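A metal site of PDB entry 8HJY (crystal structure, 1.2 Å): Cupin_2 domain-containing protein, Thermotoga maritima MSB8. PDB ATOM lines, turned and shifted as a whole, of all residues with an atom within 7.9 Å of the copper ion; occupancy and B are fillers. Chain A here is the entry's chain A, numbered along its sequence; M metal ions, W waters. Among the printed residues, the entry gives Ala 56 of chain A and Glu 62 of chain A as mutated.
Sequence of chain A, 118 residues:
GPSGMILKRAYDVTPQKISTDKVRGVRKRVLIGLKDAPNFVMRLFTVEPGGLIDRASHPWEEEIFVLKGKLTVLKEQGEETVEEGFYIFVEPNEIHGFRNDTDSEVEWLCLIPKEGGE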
ATOM      1  N   ARG A  43       2.153  20.847 -30.798  1.00  0.00           N
ATOM      2  CA  ARG A  43       3.201  21.692 -30.280  1.00  0.00           C
ATOM      3  C   ARG A  43       3.311  21.540 -28.756  1.00  0.00           C
ATOM      4  O   ARG A  43       2.309  21.271 -28.130  1.00  0.00           O
ATOM      5  CB  ARG A  43       2.988  23.163 -30.628  1.00  0.00           C
ATOM      6  CG  ARG A  43       2.814  23.446 -32.128  1.00  0.00           C
ATOM      7  CD  ARG A  43       1.389  23.358 -32.580  1.00  0.00           C
ATOM      8  NE  ARG A  43       0.376  24.153 -31.886  1.00  0.00           N
ATOM      9  CZ  ARG A  43       0.182  25.448 -32.017  1.00  0.00           C
ATOM     10  NH1 ARG A  43      -0.765  26.139 -31.370  1.00  0.00           N
ATOM     11  NH2 ARG A  43       0.927  26.168 -32.847  1.00  0.00           N
ATOM     12  N   PHE A  45       4.438  23.913 -25.674  1.00  0.00           N
ATOM     13  CA  PHE A  45       4.754  25.264 -25.250  1.00  0.00           C
ATOM     14  C   PHE A  45       5.385  25.239 -23.854  1.00  0.00           C
ATOM     15  O   PHE A  45       4.912  24.503 -23.001  1.00  0.00           O
ATOM     16  CB  PHE A  45       3.500  26.137 -25.225  1.00  0.00           C
ATOM     17  CG  PHE A  45       3.083  26.645 -26.553  1.00  0.00           C
ATOM     18  CD1 PHE A  45       3.454  27.902 -26.998  1.00  0.00           C
ATOM     19  CD2 PHE A  45       2.351  25.893 -27.439  1.00  0.00           C
ATOM     20  CE1 PHE A  45       3.111  28.382 -28.259  1.00  0.00           C
ATOM     21  CE2 PHE A  45       1.951  26.384 -28.666  1.00  0.00           C
ATOM     22  CZ  PHE A  45       2.333  27.639 -29.076  1.00  0.00           C
ATOM     23  N   ILE A  53       0.970  35.198 -22.773  1.00  0.00           N
ATOM     24  CA  ILE A  53       0.304  35.130 -24.058  1.00  0.00           C
ATOM     25  C   ILE A  53      -0.990  35.906 -23.882  1.00  0.00           C
ATOM     26  O   ILE A  53      -1.905  35.470 -23.239  1.00  0.00           O
ATOM     27  CB  ILE A  53       0.044  33.690 -24.502  1.00  0.00           C
ATOM     28  CG1 ILE A  53       1.379  32.943 -24.656  1.00  0.00           C
ATOM     29  CG2 ILE A  53      -0.774  33.670 -25.775  1.00  0.00           C
ATOM     30  CD1 ILE A  53       1.212  31.476 -24.900  1.00  0.00           C
ATOM     31  N   ASP A  54      -1.017  37.128 -24.377  1.00  0.00           N
ATOM     32  CA  ASP A  54      -2.163  37.993 -24.044  1.00  0.00           C
ATOM     33  C   ASP A  54      -3.394  37.499 -24.788  1.00  0.00           C
ATOM     34  O   ASP A  54      -3.349  36.750 -25.756  1.00  0.00           O
ATOM     35  CB  ASP A  54      -1.878  39.450 -24.329  1.00  0.00           C
ATOM     36  CG  ASP A  54      -2.458  40.303 -23.199  1.00  0.00           C
ATOM     37  OD1 ASP A  54      -3.380  39.905 -22.456  1.00  0.00           O
ATOM     38  OD2 ASP A  54      -1.929  41.389 -23.028  1.00  0.00           O
ATOM     39  N   ALA A  56      -6.362  36.793 -27.007  1.00  0.00           N
ATOM     40  CA  ALA A  56      -6.556  36.829 -28.446  1.00  0.00           C
ATOM     41  C   ALA A  56      -7.616  35.837 -28.853  1.00  0.00           C
ATOM     42  O   ALA A  56      -8.095  35.047 -28.030  1.00  0.00           O
ATOM     43  CB  ALA A  56      -5.234  36.511 -29.156  1.00  0.00           C
ATOM     44  N   SER A  57      -7.967  35.871 -30.120  1.00  0.00           N
ATOM     45  CA  SER A  57      -8.848  34.853 -30.637  1.00  0.00           C
ATOM     46  C   SER A  57      -8.440  34.571 -32.087  1.00  0.00           C
ATOM     47  O   SER A  57      -7.741  35.364 -32.705  1.00  0.00           O
ATOM     48  CB  SER A  57     -10.300  35.227 -30.580  1.00  0.00           C
ATOM     49  OG  SER A  57     -10.517  36.425 -31.300  1.00  0.00           O
ATOM     50  N   HIS A  58      -8.846  33.424 -32.583  1.00  0.00           N
ATOM     51  CA  HIS A  58      -8.489  33.066 -33.951  1.00  0.00           C
ATOM     52  C   HIS A  58      -9.571  32.141 -34.515  1.00  0.00           C
ATOM     53  O   HIS A  58     -10.301  31.510 -33.750  1.00  0.00           O
ATOM     54  CB  HIS A  58      -7.135  32.401 -34.083  1.00  0.00           C
ATOM     55  CG  HIS A  58      -6.792  31.538 -32.935  1.00  0.00           C
ATOM     56  ND1 HIS A  58      -7.437  30.352 -32.675  1.00  0.00           N
ATOM     57  CD2 HIS A  58      -5.834  31.649 -31.991  1.00  0.00           C
ATOM     58  CE1 HIS A  58      -6.883  29.772 -31.594  1.00  0.00           C
ATOM     59  NE2 HIS A  58      -5.912  30.549 -31.159  1.00  0.00           N
ATOM     60  N   TRP A  60      -9.876  29.178 -35.623  1.00  0.00           N
ATOM     61  CA  TRP A  60      -9.754  27.756 -35.465  1.00  0.00           C
ATOM     62  C   TRP A  60      -9.798  27.434 -33.968  1.00  0.00           C
ATOM     63  O   TRP A  60      -9.486  28.295 -33.147  1.00  0.00           O
ATOM     64  CB  TRP A  60      -8.478  27.192 -36.079  1.00  0.00           C
ATOM     65  CG  TRP A  60      -7.227  27.856 -35.603  1.00  0.00           C
ATOM     66  CD1 TRP A  60      -6.452  27.588 -34.514  1.00  0.00           C
ATOM     67  CD2 TRP A  60      -6.563  28.956 -36.251  1.00  0.00           C
ATOM     68  NE1 TRP A  60      -5.375  28.435 -34.439  1.00  0.00           N
ATOM     69  CE2 TRP A  60      -5.417  29.285 -35.492  1.00  0.00           C
ATOM     70  CE3 TRP A  60      -6.838  29.682 -37.411  1.00  0.00           C
ATOM     71  CZ2 TRP A  60      -4.584  30.330 -35.884  1.00  0.00           C
ATOM     72  CZ3 TRP A  60      -6.013  30.706 -37.794  1.00  0.00           C
ATOM     73  CH2 TRP A  60      -4.881  31.019 -37.028  1.00  0.00           C
ATOM     74  N   GLU A  61     -10.156  26.219 -33.679  1.00  0.00           N
ATOM     75  CA  GLU A  61     -10.162  25.716 -32.316  1.00  0.00           C
ATOM     76  C   GLU A  61      -8.746  25.396 -31.863  1.00  0.00           C
ATOM     77  O   GLU A  61      -7.813  25.227 -32.641  1.00  0.00           O
ATOM     78  CB  GLU A  61     -11.026  24.468 -32.215  1.00  0.00           C
ATOM     79  CG  GLU A  61     -10.457  23.199 -32.839  1.00  0.00           C
ATOM     80  CD  GLU A  61     -10.590  23.059 -34.321  1.00  0.00           C
ATOM     81  OE1 GLU A  61     -10.945  24.047 -35.050  1.00  0.00           O
ATOM     82  OE2 GLU A  61     -10.338  21.925 -34.801  1.00  0.00           O
ATOM     83  N   GLU A  62      -8.610  25.198 -30.548  1.00  0.00           N
ATOM     84  CA  GLU A  62      -7.402  24.750 -29.910  1.00  0.00           C
ATOM     85  C   GLU A  62      -7.710  23.695 -28.860  1.00  0.00           C
ATOM     86  O   GLU A  62      -8.663  23.854 -28.087  1.00  0.00           O
ATOM     87  CB  GLU A  62      -6.699  25.957 -29.293  1.00  0.00           C
ATOM     88  CG  GLU A  62      -5.325  25.814 -28.811  1.00  0.00           C
ATOM     89  CD  GLU A  62      -4.620  27.139 -28.599  1.00  0.00           C
ATOM     90  OE1 GLU A  62      -3.452  27.081 -28.167  1.00  0.00           O
ATOM     91  OE2 GLU A  62      -5.177  28.218 -28.904  1.00  0.00           O
ATOM     92  N   ILE A  64      -5.817  21.640 -25.734  1.00  0.00           N
ATOM     93  CA  ILE A  64      -4.679  21.766 -24.850  1.00  0.00           C
ATOM     94  C   ILE A  64      -4.687  20.685 -23.767  1.00  0.00           C
ATOM     95  O   ILE A  64      -5.722  20.340 -23.219  1.00  0.00           O
ATOM     96  CB  ILE A  64      -4.689  23.172 -24.216  1.00  0.00           C
ATOM     97  CG1 ILE A  64      -4.384  24.200 -25.319  1.00  0.00           C
ATOM     98  CG2 ILE A  64      -3.730  23.306 -23.042  1.00  0.00           C
ATOM     99  CD1 ILE A  64      -4.787  25.591 -24.881  1.00  0.00           C
ATOM    100  N   VAL A  90     -10.723  25.177 -26.537  1.00  0.00           N
ATOM    101  CA  VAL A  90     -11.025  26.566 -26.897  1.00  0.00           C
ATOM    102  C   VAL A  90     -11.763  26.548 -28.240  1.00  0.00           C
ATOM    103  O   VAL A  90     -11.204  26.119 -29.256  1.00  0.00           O
ATOM    104  CB  VAL A  90      -9.750  27.411 -27.001  1.00  0.00           C
ATOM    105  CG1 VAL A  90     -10.120  28.891 -27.157  1.00  0.00           C
ATOM    106  CG2 VAL A  90      -8.789  27.253 -25.819  1.00  0.00           C
ATOM    107  N   GLU A  94     -13.093  32.013 -29.649  1.00  0.00           N
ATOM    108  CA  GLU A  94     -13.189  32.293 -28.216  1.00  0.00           C
ATOM    109  C   GLU A  94     -11.942  33.013 -27.754  1.00  0.00           C
ATOM    110  O   GLU A  94     -10.813  32.624 -28.017  1.00  0.00           O
ATOM    111  CB  GLU A  94     -13.379  30.987 -27.459  1.00  0.00           C
ATOM    112  CG  GLU A  94     -13.653  31.166 -25.981  1.00  0.00           C
ATOM    113  CD  GLU A  94     -14.970  31.882 -25.725  1.00  0.00           C
ATOM    114  OE1 GLU A  94     -15.006  32.807 -24.870  1.00  0.00           O
ATOM    115  OE2 GLU A  94     -15.969  31.547 -26.426  1.00  0.00           O
ATOM    116  N   ILE A  95     -12.107  34.084 -26.991  1.00  0.00           N
ATOM    117  CA  ILE A  95     -11.008  34.787 -26.376  1.00  0.00           C
ATOM    118  C   ILE A  95     -10.294  33.957 -25.333  1.00  0.00           C
ATOM    119  O   ILE A  95     -10.919  33.319 -24.471  1.00  0.00           O
ATOM    120  CB  ILE A  95     -11.515  36.108 -25.735  1.00  0.00           C
ATOM    121  CG1 ILE A  95     -12.033  37.027 -26.826  1.00  0.00           C
ATOM    122  CG2 ILE A  95     -10.439  36.765 -24.903  1.00  0.00           C
ATOM    123  CD1 ILE A  95     -12.886  38.174 -26.314  1.00  0.00           C
ATOM    124  N   HIS A  96      -8.965  33.931 -25.419  1.00  0.00           N
ATOM    125  CA  HIS A  96      -8.167  33.134 -24.500  1.00  0.00           C
ATOM    126  C   HIS A  96      -6.753  33.715 -24.471  1.00  0.00           C
ATOM    127  O   HIS A  96      -6.302  34.310 -25.427  1.00  0.00           O
ATOM    128  CB  HIS A  96      -8.116  31.661 -24.917  1.00  0.00           C
ATOM    129  CG  HIS A  96      -7.513  31.455 -26.259  1.00  0.00           C
ATOM    130  ND1 HIS A  96      -8.125  31.837 -27.398  1.00  0.00           N
ATOM    131  CD2 HIS A  96      -6.319  30.912 -26.638  1.00  0.00           C
ATOM    132  CE1 HIS A  96      -7.367  31.510 -28.410  1.00  0.00           C
ATOM    133  NE2 HIS A  96      -6.245  30.978 -28.015  1.00  0.00           N
ATOM    134  N   GLY A  97      -6.072  33.489 -23.362  1.00  0.00           N
ATOM    135  CA  GLY A  97      -4.657  33.774 -23.219  1.00  0.00           C
ATOM    136  C   GLY A  97      -4.113  33.041 -22.006  1.00  0.00           C
ATOM    137  O   GLY A  97      -4.870  32.278 -21.387  1.00  0.00           O
ATOM    138  N   PHE A  98      -2.842  33.231 -21.714  1.00  0.00           N
ATOM    139  CA  PHE A  98      -2.163  32.399 -20.725  1.00  0.00           C
ATOM    140  C   PHE A  98      -1.100  33.222 -20.002  1.00  0.00           C
ATOM    141  O   PHE A  98      -0.452  34.088 -20.609  1.00  0.00           O
ATOM    142  CB  PHE A  98      -1.486  31.186 -21.340  1.00  0.00           C
ATOM    143  CG  PHE A  98      -2.473  30.379 -22.124  1.00  0.00           C
ATOM    144  CD1 PHE A  98      -3.330  29.499 -21.487  1.00  0.00           C
ATOM    145  CD2 PHE A  98      -2.533  30.503 -23.483  1.00  0.00           C
ATOM    146  CE1 PHE A  98      -4.218  28.778 -22.245  1.00  0.00           C
ATOM    147  CE2 PHE A  98      -3.452  29.783 -24.262  1.00  0.00           C
ATOM    148  CZ  PHE A  98      -4.303  28.911 -23.624  1.00  0.00           C
ATOM    149  N   CYS A 110      -0.325  21.776 -27.171  1.00  0.00           N
ATOM    150  CA  CYS A 110      -1.337  22.510 -27.901  1.00  0.00           C
ATOM    151  C   CYS A 110      -1.473  21.919 -29.303  1.00  0.00           C
ATOM    152  O   CYS A 110      -0.478  21.820 -30.024  1.00  0.00           O
ATOM    153  CB  CYS A 110      -0.979  23.994 -27.997  1.00  0.00           C
ATOM    154  SG  CYS A 110      -2.218  24.817 -29.003  1.00  0.00           S
ATOM    155  N   ILE A 112      -3.808  22.205 -32.950  1.00  0.00           N
ATOM    156  CA  ILE A 112      -4.678  23.016 -33.788  1.00  0.00           C
ATOM    157  C   ILE A 112      -4.818  22.330 -35.133  1.00  0.00           C
ATOM    158  O   ILE A 112      -3.889  21.643 -35.576  1.00  0.00           O
ATOM    159  CB  ILE A 112      -4.179  24.476 -33.922  1.00  0.00           C
ATOM    160  CG1 ILE A 112      -2.811  24.583 -34.592  1.00  0.00           C
ATOM    161  CG2 ILE A 112      -4.224  25.189 -32.595  1.00  0.00           C
ATOM    162  CD1 ILE A 112      -2.385  26.026 -34.895  1.00  0.00           C
HETATM  163 CU    CU M   1      -4.838  30.461 -29.400  1.00  0.00          CU
HETATM  164  O   HOH W   1      -3.020  30.583 -27.830  1.00  0.00           O
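O of His 96 is in hydrogen-bond range of N of Ala 56 (2.9 Å). ND1 of His 96 is in hydrogen-bond range of O of Glu 94. ND1 of His 58 sits at hydrogen-bond distance from O of Trp 60 (2.9 Å). The backbone NH (N) of Val 90 is in hydrogen-bond range of the backbone carbonyl oxygen (O) of Glu 62, at 2.9 Å. OE1 of Glu 62 lies within hydrogen-bond range of SG of Cys 110, at 2.7 Å.
Three residues have an atom within 4 Å of the copper ion: His 58, Glu 62 and His 96. The nearest printed residue that does not touch the copper ion is Phe 98 (5.4 Å).
NE2 of His 96 binds the copper ion (2.0 Å). NE2 of His 58 is bound to the copper ion. The copper ion is bound by OE2 of Glu 62 (2.3 Å). The copper ion is bound by water W1, at 2.4 Å.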
